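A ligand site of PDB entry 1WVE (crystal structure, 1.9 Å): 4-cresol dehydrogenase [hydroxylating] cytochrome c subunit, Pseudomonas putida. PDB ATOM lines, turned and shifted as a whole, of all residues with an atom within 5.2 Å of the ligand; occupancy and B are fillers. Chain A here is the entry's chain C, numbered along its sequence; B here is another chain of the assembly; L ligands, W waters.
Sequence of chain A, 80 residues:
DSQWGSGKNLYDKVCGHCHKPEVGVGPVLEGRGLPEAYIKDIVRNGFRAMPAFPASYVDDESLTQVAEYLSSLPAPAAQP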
ATOM      1  N   LEU A  10      -7.062  27.399  35.941  1.00  0.00           N
ATOM      2  CA  LEU A  10      -6.560  26.079  35.546  1.00  0.00           C
ATOM      3  C   LEU A  10      -5.434  26.283  34.538  1.00  0.00           C
ATOM      4  O   LEU A  10      -4.374  25.649  34.614  1.00  0.00           O
ATOM      5  CB  LEU A  10      -7.657  25.236  34.898  1.00  0.00           C
ATOM      6  CG  LEU A  10      -7.128  23.941  34.256  1.00  0.00           C
ATOM      7  CD1 LEU A  10      -6.492  23.059  35.334  1.00  0.00           C
ATOM      8  CD2 LEU A  10      -8.261  23.198  33.548  1.00  0.00           C
ATOM      9  N   VAL A  14      -1.766  25.020  35.484  1.00  0.00           N
ATOM     10  CA  VAL A  14      -1.428  23.760  34.838  1.00  0.00           C
ATOM     11  C   VAL A  14      -1.066  23.881  33.354  1.00  0.00           C
ATOM     12  O   VAL A  14       0.121  23.946  32.998  1.00  0.00           O
ATOM     13  CB  VAL A  14      -2.611  22.738  34.977  1.00  0.00           C
ATOM     14  CG1 VAL A  14      -2.250  21.408  34.336  1.00  0.00           C
ATOM     15  CG2 VAL A  14      -2.954  22.543  36.435  1.00  0.00           C
ATOM     16  N   CYS A  15      -2.071  23.944  32.500  1.00  0.00           N
ATOM     17  CA  CYS A  15      -1.869  23.998  31.050  1.00  0.00           C
ATOM     18  C   CYS A  15      -0.887  25.041  30.538  1.00  0.00           C
ATOM     19  O   CYS A  15      -0.080  24.752  29.660  1.00  0.00           O
ATOM     20  CB  CYS A  15      -3.192  24.207  30.315  1.00  0.00           C
ATOM     21  SG  CYS A  15      -4.631  23.419  31.099  1.00  0.00           S
ATOM     22  N   CYS A  18       3.018  24.899  29.990  1.00  0.00           N
ATOM     23  CA  CYS A  18       3.515  24.269  28.780  1.00  0.00           C
ATOM     24  C   CYS A  18       3.020  24.965  27.531  1.00  0.00           C
ATOM     25  O   CYS A  18       3.762  25.100  26.560  1.00  0.00           O
ATOM     26  CB  CYS A  18       3.082  22.808  28.716  1.00  0.00           C
ATOM     27  SG  CYS A  18       3.903  21.720  29.914  1.00  0.00           S
ATOM     28  N   HIS A  19       1.755  25.399  27.566  1.00  0.00           N
ATOM     29  CA  HIS A  19       1.117  26.010  26.413  1.00  0.00           C
ATOM     30  C   HIS A  19       1.210  27.531  26.194  1.00  0.00           C
ATOM     31  O   HIS A  19       0.966  27.998  25.074  1.00  0.00           O
ATOM     32  CB  HIS A  19      -0.367  25.583  26.372  1.00  0.00           C
ATOM     33  CG  HIS A  19      -0.569  24.175  25.908  1.00  0.00           C
ATOM     34  ND1 HIS A  19      -0.469  23.849  24.592  1.00  0.00           N
ATOM     35  CD2 HIS A  19      -0.831  23.201  26.829  1.00  0.00           C
ATOM     36  CE1 HIS A  19      -0.690  22.489  24.631  1.00  0.00           C
ATOM     37  NE2 HIS A  19      -0.919  22.064  25.970  1.00  0.00           N
ATOM     38  N   VAL A  25       6.255  24.674  25.033  1.00  0.00           N
ATOM     39  CA  VAL A  25       6.418  23.219  25.141  1.00  0.00           C
ATOM     40  C   VAL A  25       5.315  22.574  24.312  1.00  0.00           C
ATOM     41  O   VAL A  25       5.545  21.594  23.600  1.00  0.00           O
ATOM     42  CB  VAL A  25       6.324  22.738  26.618  1.00  0.00           C
ATOM     43  CG1 VAL A  25       6.117  21.221  26.667  1.00  0.00           C
ATOM     44  CG2 VAL A  25       7.604  23.114  27.362  1.00  0.00           C
ATOM     45  N   GLY A  26       4.117  23.128  24.427  1.00  0.00           N
ATOM     46  CA  GLY A  26       2.985  22.621  23.677  1.00  0.00           C
ATOM     47  C   GLY A  26       2.506  23.713  22.743  1.00  0.00           C
ATOM     48  O   GLY A  26       2.872  24.875  22.921  1.00  0.00           O
ATOM     49  N   PRO A  27       1.676  23.392  21.744  1.00  0.00           N
ATOM     50  CA  PRO A  27       1.188  24.421  20.817  1.00  0.00           C
ATOM     51  C   PRO A  27       0.283  25.474  21.468  1.00  0.00           C
ATOM     52  O   PRO A  27      -0.311  25.230  22.533  1.00  0.00           O
ATOM     53  CB  PRO A  27       0.479  23.616  19.728  1.00  0.00           C
ATOM     54  CG  PRO A  27      -0.015  22.390  20.494  1.00  0.00           C
ATOM     55  CD  PRO A  27       1.164  22.061  21.380  1.00  0.00           C
ATOM     56  N   LEU A  29      -2.849  27.505  22.347  1.00  0.00           N
ATOM     57  CA  LEU A  29      -4.263  27.133  22.418  1.00  0.00           C
ATOM     58  C   LEU A  29      -5.142  28.378  22.511  1.00  0.00           C
ATOM     59  O   LEU A  29      -6.343  28.309  22.323  1.00  0.00           O
ATOM     60  CB  LEU A  29      -4.512  26.270  23.668  1.00  0.00           C
ATOM     61  CG  LEU A  29      -3.595  25.077  23.916  1.00  0.00           C
ATOM     62  CD1 LEU A  29      -3.989  24.429  25.252  1.00  0.00           C
ATOM     63  CD2 LEU A  29      -3.689  24.070  22.780  1.00  0.00           C
ATOM     64  N   LEU A  34     -10.629  25.964  19.734  1.00  0.00           N
ATOM     65  CA  LEU A  34     -10.623  24.522  19.979  1.00  0.00           C
ATOM     66  C   LEU A  34     -11.905  24.090  20.711  1.00  0.00           C
ATOM     67  O   LEU A  34     -12.233  24.628  21.769  1.00  0.00           O
ATOM     68  CB  LEU A  34      -9.386  24.124  20.801  1.00  0.00           C
ATOM     69  CG  LEU A  34      -8.032  24.453  20.157  1.00  0.00           C
ATOM     70  CD1 LEU A  34      -6.902  24.224  21.161  1.00  0.00           C
ATOM     71  CD2 LEU A  34      -7.820  23.582  18.928  1.00  0.00           C
ATOM     72  N   TYR A  38     -12.787  18.283  21.985  1.00  0.00           N
ATOM     73  CA  TYR A  38     -11.399  17.987  21.609  1.00  0.00           C
ATOM     74  C   TYR A  38     -10.457  18.170  22.800  1.00  0.00           C
ATOM     75  O   TYR A  38      -9.579  17.347  23.041  1.00  0.00           O
ATOM     76  CB  TYR A  38     -10.939  18.909  20.475  1.00  0.00           C
ATOM     77  CG  TYR A  38      -9.533  18.628  20.002  1.00  0.00           C
ATOM     78  CD1 TYR A  38      -9.200  17.388  19.434  1.00  0.00           C
ATOM     79  CD2 TYR A  38      -8.528  19.590  20.095  1.00  0.00           C
ATOM     80  CE1 TYR A  38      -7.918  17.120  18.967  1.00  0.00           C
ATOM     81  CE2 TYR A  38      -7.229  19.337  19.636  1.00  0.00           C
ATOM     82  CZ  TYR A  38      -6.935  18.098  19.082  1.00  0.00           C
ATOM     83  OH  TYR A  38      -5.671  17.817  18.615  1.00  0.00           O
ATOM     84  N   ILE A  39     -10.633  19.255  23.542  1.00  0.00           N
ATOM     85  CA  ILE A  39      -9.812  19.515  24.718  1.00  0.00           C
ATOM     86  C   ILE A  39      -9.979  18.386  25.758  1.00  0.00           C
ATOM     87  O   ILE A  39      -8.990  17.903  26.296  1.00  0.00           O
ATOM     88  CB  ILE A  39     -10.195  20.875  25.335  1.00  0.00           C
ATOM     89  CG1 ILE A  39      -9.709  21.986  24.391  1.00  0.00           C
ATOM     90  CG2 ILE A  39      -9.584  21.017  26.723  1.00  0.00           C
ATOM     91  CD1 ILE A  39     -10.157  23.376  24.762  1.00  0.00           C
ATOM     92  N   ILE A  42      -8.149  15.260  24.476  1.00  0.00           N
ATOM     93  CA  ILE A  42      -6.686  15.372  24.571  1.00  0.00           C
ATOM     94  C   ILE A  42      -6.211  15.256  26.026  1.00  0.00           C
ATOM     95  O   ILE A  42      -5.228  14.580  26.304  1.00  0.00           O
ATOM     96  CB  ILE A  42      -6.181  16.725  23.990  1.00  0.00           C
ATOM     97  CG1 ILE A  42      -6.346  16.735  22.465  1.00  0.00           C
ATOM     98  CG2 ILE A  42      -4.706  16.954  24.391  1.00  0.00           C
ATOM     99  CD1 ILE A  42      -5.410  15.794  21.711  1.00  0.00           C
ATOM    100  N   VAL A  43      -6.925  15.909  26.945  1.00  0.00           N
ATOM    101  CA  VAL A  43      -6.532  15.874  28.348  1.00  0.00           C
ATOM    102  C   VAL A  43      -6.745  14.484  28.974  1.00  0.00           C
ATOM    103  O   VAL A  43      -5.890  14.017  29.726  1.00  0.00           O
ATOM    104  CB  VAL A  43      -7.303  16.933  29.160  1.00  0.00           C
ATOM    105  CG1 VAL A  43      -6.980  16.816  30.651  1.00  0.00           C
ATOM    106  CG2 VAL A  43      -6.910  18.334  28.671  1.00  0.00           C
ATOM    107  N   PHE A  47      -1.596  12.952  24.803  1.00  0.00           N
ATOM    108  CA  PHE A  47      -1.331  12.950  23.362  1.00  0.00           C
ATOM    109  C   PHE A  47       0.151  13.028  23.077  1.00  0.00           C
ATOM    110  O   PHE A  47       0.752  14.092  23.137  1.00  0.00           O
ATOM    111  CB  PHE A  47      -2.060  14.108  22.680  1.00  0.00           C
ATOM    112  CG  PHE A  47      -1.884  14.118  21.175  1.00  0.00           C
ATOM    113  CD1 PHE A  47      -2.094  12.959  20.439  1.00  0.00           C
ATOM    114  CD2 PHE A  47      -1.493  15.272  20.509  1.00  0.00           C
ATOM    115  CE1 PHE A  47      -1.903  12.940  19.053  1.00  0.00           C
ATOM    116  CE2 PHE A  47      -1.299  15.264  19.130  1.00  0.00           C
ATOM    117  CZ  PHE A  47      -1.500  14.101  18.397  1.00  0.00           C
ATOM    118  N   ARG A  48       0.720  11.873  22.759  1.00  0.00           N
ATOM    119  CA  ARG A  48       2.138  11.786  22.461  1.00  0.00           C
ATOM    120  C   ARG A  48       2.967  12.424  23.572  1.00  0.00           C
ATOM    121  O   ARG A  48       2.971  11.913  24.683  1.00  0.00           O
ATOM    122  CB  ARG A  48       2.427  12.417  21.100  1.00  0.00           C
ATOM    123  CG  ARG A  48       1.769  11.601  19.982  1.00  0.00           C
ATOM    124  CD  ARG A  48       1.959  12.223  18.595  1.00  0.00           C
ATOM    125  NE  ARG A  48       1.222  11.462  17.582  1.00  0.00           N
ATOM    126  CZ  ARG A  48       1.007  11.874  16.336  1.00  0.00           C
ATOM    127  NH1 ARG A  48       1.482  13.049  15.934  1.00  0.00           N
ATOM    128  NH2 ARG A  48       0.313  11.124  15.488  1.00  0.00           N
ATOM    129  N   ALA A  49       3.656  13.529  23.295  1.00  0.00           N
ATOM    130  CA  ALA A  49       4.487  14.160  24.324  1.00  0.00           C
ATOM    131  C   ALA A  49       3.675  14.712  25.491  1.00  0.00           C
ATOM    132  O   ALA A  49       4.197  14.901  26.592  1.00  0.00           O
ATOM    133  CB  ALA A  49       5.347  15.282  23.700  1.00  0.00           C
ATOM    134  N   MET A  50       2.402  14.988  25.255  1.00  0.00           N
ATOM    135  CA  MET A  50       1.555  15.514  26.317  1.00  0.00           C
ATOM    136  C   MET A  50       0.983  14.459  27.249  1.00  0.00           C
ATOM    137  O   MET A  50       0.392  13.482  26.800  1.00  0.00           O
ATOM    138  CB  MET A  50       0.379  16.297  25.767  1.00  0.00           C
ATOM    139  CG  MET A  50      -0.440  16.920  26.921  1.00  0.00           C
ATOM    140  SD  MET A  50      -1.850  17.870  26.372  1.00  0.00           S
ATOM    141  CE  MET A  50      -2.999  17.501  27.694  1.00  0.00           C
ATOM    142  N   PRO A  51       1.141  14.663  28.555  1.00  0.00           N
ATOM    143  CA  PRO A  51       0.612  13.714  29.547  1.00  0.00           C
ATOM    144  C   PRO A  51      -0.915  13.772  29.642  1.00  0.00           C
ATOM    145  O   PRO A  51      -1.551  14.712  29.163  1.00  0.00           O
ATOM    146  CB  PRO A  51       1.295  14.136  30.848  1.00  0.00           C
ATOM    147  CG  PRO A  51       1.590  15.583  30.646  1.00  0.00           C
ATOM    148  CD  PRO A  51       1.966  15.701  29.187  1.00  0.00           C
ATOM    149  N   PHE A  53      -4.388  13.627  32.149  1.00  0.00           N
ATOM    150  CA  PHE A  53      -4.758  14.040  33.494  1.00  0.00           C
ATOM    151  C   PHE A  53      -6.065  13.378  33.901  1.00  0.00           C
ATOM    152  O   PHE A  53      -7.082  13.505  33.205  1.00  0.00           O
ATOM    153  CB  PHE A  53      -4.945  15.565  33.594  1.00  0.00           C
ATOM    154  CG  PHE A  53      -3.657  16.338  33.543  1.00  0.00           C
ATOM    155  CD1 PHE A  53      -3.084  16.662  32.311  1.00  0.00           C
ATOM    156  CD2 PHE A  53      -2.995  16.696  34.712  1.00  0.00           C
ATOM    157  CE1 PHE A  53      -1.857  17.327  32.251  1.00  0.00           C
ATOM    158  CE2 PHE A  53      -1.772  17.367  34.671  1.00  0.00           C
ATOM    159  CZ  PHE A  53      -1.189  17.687  33.441  1.00  0.00           C
ATOM    160  N   VAL A  58      -7.963  17.078  37.140  1.00  0.00           N
ATOM    161  CA  VAL A  58      -8.664  18.123  36.382  1.00  0.00           C
ATOM    162  C   VAL A  58     -10.024  17.570  35.967  1.00  0.00           C
ATOM    163  O   VAL A  58     -10.124  16.783  35.026  1.00  0.00           O
ATOM    164  CB  VAL A  58      -7.880  18.519  35.112  1.00  0.00           C
ATOM    165  CG1 VAL A  58      -8.590  19.673  34.403  1.00  0.00           C
ATOM    166  CG2 VAL A  58      -6.471  18.916  35.468  1.00  0.00           C
ATOM    167  N   LEU A  63     -12.534  21.527  32.611  1.00  0.00           N
ATOM    168  CA  LEU A  63     -12.183  21.437  31.203  1.00  0.00           C
ATOM    169  C   LEU A  63     -13.164  22.301  30.397  1.00  0.00           C
ATOM    170  O   LEU A  63     -12.782  22.963  29.427  1.00  0.00           O
ATOM    171  CB  LEU A  63     -12.227  19.975  30.742  1.00  0.00           C
ATOM    172  CG  LEU A  63     -10.892  19.196  30.691  1.00  0.00           C
ATOM    173  CD1 LEU A  63      -9.834  19.872  31.491  1.00  0.00           C
ATOM    174  CD2 LEU A  63     -11.113  17.778  31.164  1.00  0.00           C
ATOM    175  N   VAL A  66     -11.911  25.878  30.942  1.00  0.00           N
ATOM    176  CA  VAL A  66     -10.686  26.253  30.228  1.00  0.00           C
ATOM    177  C   VAL A  66     -10.957  26.327  28.728  1.00  0.00           C
ATOM    178  O   VAL A  66     -10.394  27.169  28.032  1.00  0.00           O
ATOM    179  CB  VAL A  66      -9.509  25.269  30.554  1.00  0.00           C
ATOM    180  CG1 VAL A  66      -9.622  23.987  29.768  1.00  0.00           C
ATOM    181  CG2 VAL A  66      -8.174  25.966  30.323  1.00  0.00           C
ATOM    182  N   LEU A  70     -10.044  29.711  26.833  1.00  0.00           N
ATOM    183  CA  LEU A  70      -9.098  29.761  25.723  1.00  0.00           C
ATOM    184  C   LEU A  70      -9.727  30.304  24.445  1.00  0.00           C
ATOM    185  O   LEU A  70      -9.091  31.065  23.725  1.00  0.00           O
ATOM    186  CB  LEU A  70      -8.485  28.386  25.473  1.00  0.00           C
ATOM    187  CG  LEU A  70      -7.644  27.901  26.654  1.00  0.00           C
ATOM    188  CD1 LEU A  70      -7.211  26.450  26.448  1.00  0.00           C
ATOM    189  CD2 LEU A  70      -6.424  28.811  26.793  1.00  0.00           C
ATOM    190  N   ILE B 157       3.173  20.635  38.772  1.00  0.00           N
ATOM    191  CA  ILE B 157       2.189  19.558  38.794  1.00  0.00           C
ATOM    192  C   ILE B 157       2.574  18.326  39.596  1.00  0.00           C
ATOM    193  O   ILE B 157       1.739  17.481  39.891  1.00  0.00           O
ATOM    194  CB  ILE B 157       1.793  19.111  37.361  1.00  0.00           C
ATOM    195  CG1 ILE B 157       3.026  18.632  36.600  1.00  0.00           C
ATOM    196  CG2 ILE B 157       1.108  20.259  36.637  1.00  0.00           C
ATOM    197  CD1 ILE B 157       2.695  18.119  35.190  1.00  0.00           C
ATOM    198  N   LEU B 377       7.634  24.364  33.649  1.00  0.00           N
ATOM    199  CA  LEU B 377       7.714  23.072  32.997  1.00  0.00           C
ATOM    200  C   LEU B 377       8.552  23.171  31.725  1.00  0.00           C
ATOM    201  O   LEU B 377       8.404  22.368  30.802  1.00  0.00           O
ATOM    202  CB  LEU B 377       6.303  22.535  32.685  1.00  0.00           C
ATOM    203  CG  LEU B 377       5.404  22.336  33.925  1.00  0.00           C
ATOM    204  CD1 LEU B 377       4.064  21.694  33.530  1.00  0.00           C
ATOM    205  CD2 LEU B 377       6.107  21.479  34.911  1.00  0.00           C
ATOM    206  N   PHE B 380      10.147  20.137  29.827  1.00  0.00           N
ATOM    207  CA  PHE B 380       9.371  19.154  29.091  1.00  0.00           C
ATOM    208  C   PHE B 380       9.672  19.282  27.593  1.00  0.00           C
ATOM    209  O   PHE B 380       9.190  18.493  26.786  1.00  0.00           O
ATOM    210  CB  PHE B 380       7.882  19.294  29.401  1.00  0.00           C
ATOM    211  CG  PHE B 380       7.452  18.554  30.643  1.00  0.00           C
ATOM    212  CD1 PHE B 380       6.674  17.397  30.558  1.00  0.00           C
ATOM    213  CD2 PHE B 380       7.847  19.000  31.905  1.00  0.00           C
ATOM    214  CE1 PHE B 380       6.289  16.696  31.721  1.00  0.00           C
ATOM    215  CE2 PHE B 380       7.475  18.304  33.070  1.00  0.00           C
ATOM    216  CZ  PHE B 380       6.695  17.157  32.970  1.00  0.00           C
ATOM    217  N   ASN B 384      10.061  16.892  23.108  1.00  0.00           N
ATOM    218  CA  ASN B 384       9.840  17.352  21.739  1.00  0.00           C
ATOM    219  C   ASN B 384      11.090  17.089  20.892  1.00  0.00           C
ATOM    220  O   ASN B 384      11.049  17.260  19.679  1.00  0.00           O
ATOM    221  CB  ASN B 384       9.511  18.858  21.713  1.00  0.00           C
ATOM    222  CG  ASN B 384       8.182  19.175  22.391  1.00  0.00           C
ATOM    223  OD1 ASN B 384       7.310  18.317  22.534  1.00  0.00           O
ATOM    224  ND2 ASN B 384       8.011  20.439  22.789  1.00  0.00           N
ATOM    225  N   GLY B 388       6.623  11.968  19.937  1.00  0.00           N
ATOM    226  CA  GLY B 388       6.021  10.652  19.892  1.00  0.00           C
ATOM    227  C   GLY B 388       5.625  10.014  21.214  1.00  0.00           C
ATOM    228  O   GLY B 388       5.050   8.942  21.235  1.00  0.00           O
HETATM  229  C1  LIG L   1      -1.089  19.426  22.951  1.00  0.00           C
HETATM  230  C2  LIG L   1      -4.682  20.851  25.833  1.00  0.00           C
HETATM  231  C3  LIG L   1      -1.683  20.732  29.617  1.00  0.00           C
HETATM  232  C4  LIG L   1       1.946  19.618  26.696  1.00  0.00           C
HETATM  233  C5  LIG L   1      -2.344  19.802  23.390  1.00  0.00           C
HETATM  234  C6  LIG L   1      -3.537  19.930  22.565  1.00  0.00           C
HETATM  235  C7  LIG L   1      -4.539  20.334  23.361  1.00  0.00           C
HETATM  236  C8  LIG L   1      -4.002  20.463  24.707  1.00  0.00           C
HETATM  237  C9  LIG L   1      -5.996  20.613  22.984  1.00  0.00           C
HETATM  238  C10 LIG L   1      -3.567  19.659  21.059  1.00  0.00           C
HETATM  239  C11 LIG L   1      -3.469  20.979  20.296  1.00  0.00           C
HETATM  240  C12 LIG L   1      -3.488  20.831  18.796  1.00  0.00           C
HETATM  241  O1  LIG L   1      -3.044  21.859  18.168  1.00  0.00           O
HETATM  242  O2  LIG L   1      -3.903  19.781  18.307  1.00  0.00           O
HETATM  243  C13 LIG L   1      -4.181  20.949  27.108  1.00  0.00           C
HETATM  244  C14 LIG L   1      -4.943  21.377  28.260  1.00  0.00           C
HETATM  245  C15 LIG L   1      -4.099  21.321  29.327  1.00  0.00           C
HETATM  246  C16 LIG L   1      -2.822  20.889  28.847  1.00  0.00           C
HETATM  247  C17 LIG L   1      -6.425  21.803  28.236  1.00  0.00           C
HETATM  248  C18 LIG L   1      -4.361  21.651  30.783  1.00  0.00           C
HETATM  249  C19 LIG L   1      -5.357  20.677  31.473  1.00  0.00           C
HETATM  250  C20 LIG L   1      -0.422  20.418  29.149  1.00  0.00           C
HETATM  251  C21 LIG L   1       0.772  20.395  29.983  1.00  0.00           C
HETATM  252  C22 LIG L   1       1.791  20.105  29.165  1.00  0.00           C
HETATM  253  C23 LIG L   1       1.248  19.947  27.827  1.00  0.00           C
HETATM  254  C24 LIG L   1       0.785  20.692  31.510  1.00  0.00           C
HETATM  255  C25 LIG L   1       3.283  20.052  29.488  1.00  0.00           C
HETATM  256  C26 LIG L   1       3.720  18.936  30.475  1.00  0.00           C
HETATM  257  C27 LIG L   1       1.457  19.442  25.416  1.00  0.00           C
HETATM  258  C28 LIG L   1       2.232  19.065  24.261  1.00  0.00           C
HETATM  259  C29 LIG L   1       1.387  18.984  23.205  1.00  0.00           C
HETATM  260  C30 LIG L   1       0.070  19.350  23.710  1.00  0.00           C
HETATM  261  C31 LIG L   1       3.773  18.802  24.276  1.00  0.00           C
HETATM  262  C32 LIG L   1       1.759  18.564  21.777  1.00  0.00           C
HETATM  263  C33 LIG L   1       1.916  17.001  21.747  1.00  0.00           C
HETATM  264  C34 LIG L   1       2.434  16.444  20.443  1.00  0.00           C
HETATM  265  O3  LIG L   1       2.042  16.898  19.365  1.00  0.00           O
HETATM  266  O4  LIG L   1       3.287  15.542  20.577  1.00  0.00           O
HETATM  267  N1  LIG L   1      -2.659  20.128  24.687  1.00  0.00           N
HETATM  268  N2  LIG L   1      -2.861  20.678  27.490  1.00  0.00           N
HETATM  269  N3  LIG L   1      -0.114  20.139  27.835  1.00  0.00           N
HETATM  270  N4  LIG L   1       0.113  19.618  25.071  1.00  0.00           N
HETATM  271 FE1  LIG L   1      -1.377  20.112  26.270  1.00  0.00          FE
HETATM  272  O   HOH W   1       4.814  18.905  19.589  1.00  0.00           O
HETATM  273  O   HOH W   2      -1.729  18.927  16.559  1.00  0.00           O
HETATM  274  O   HOH W   3       5.220  14.288  19.274  1.00  0.00           O
HETATM  275  O   HOH W   4      -3.725  24.462  18.805  1.00  0.00           O
HETATM  276  O   HOH W   5       6.555  16.554  20.441  1.00  0.00           O
HETATM  277  O   HOH W   6       0.914  19.074  18.372  1.00  0.00           O
HETATM  278  O   HOH W   7       2.137  15.115  17.274  1.00  0.00           O
HETATM  279  O   HOH W   8       6.881  18.145  25.343  1.00  0.00           O
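ND1 of His 19 is in hydrogen-bond range of O of Pro 27 (2.5 Å). The backbone carbonyl oxygen (O) of Val 43 is in hydrogen-bond range of the backbone NH (N) of Phe 53 (2.9 Å). The backbone carbonyl oxygen (O) of Cys 18 lies within hydrogen-bond range of the backbone NH (N) of Val 25 (3.0 Å). The backbone NH (N) of Gly 26 lies within hydrogen-bond range of the backbone carbonyl oxygen (O) of Cys 18, 2.9 Å away. The backbone carbonyl oxygen (O) of Val 25 lies within hydrogen-bond range of the side-chain amide nitrogen (ND2) of Asn 384 of chain B, 2.8 Å away.
An oxygen (O2) of the ligand sits at hydrogen-bond distance from the side-chain hydroxyl of Tyr 38 (2.7 Å). C25 of the ligand is bonded to SG of Cys 18 (1.8 Å). FE1 of the ligand is bound by SD of Met 50, at 2.3 Å. The backbone NH (N) of Ala 49 sits at hydrogen-bond distance from an oxygen (O4) of the ligand (3.4 Å). NE2 of His 19 binds FE1 of the ligand (2.0 Å). The side-chain sulfur (SG) of Cys 15 is bonded to a carbon (C18) of the ligand (1.8 Å).
Residues that only touch the ligand: Val 14 (3.6 Å), Val 25 (3.4 Å), Gly 26 (3.7 Å), Pro 27 (3.6 Å), Leu 29 (3.7 Å), Ile 39 (3.6 Å), Ile 42 (3.5 Å), Val 43 (3.5 Å), Phe 47 (3.4 Å), Arg 48 (3.3 Å), Pro 51 (3.9 Å), Leu 377 of chain B (3.98 Å), Phe 380 of chain B (3.3 Å) and Asn 384 of chain B (3.97 Å). Hydrophobic or aromatic side chains that line the ligand: His 19, Pro 27, Leu 29, Tyr 38, Ile 39, Ile 42, Val 43, Phe 47, Ala 49, Met 50, Pro 51, Leu 377 of chain B and Phe 380 of chain B. The nearest printed residue that does not touch the ligand is Phe 53 (4.1 Å).
Water W3 bridges O4 of the ligand (2.6 Å) and N of Gly 388 of chain B (2.8 Å). Water W7 lies within hydrogen-bond range of the guanidinium group (NH1) of Arg 48 and an oxygen (O3) of the ligand. Water W8 lies within hydrogen-bond range of the backbone carbonyl oxygen (O) of Phe 380 of chain B (2.7 Å) and the side-chain amide oxygen (OD1) of Asn 384 of chain B (2.8 Å). Water W5 bridges OD1 of Asn 384 of chain B (2.8 Å) and O4 of the ligand (3.4 Å).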
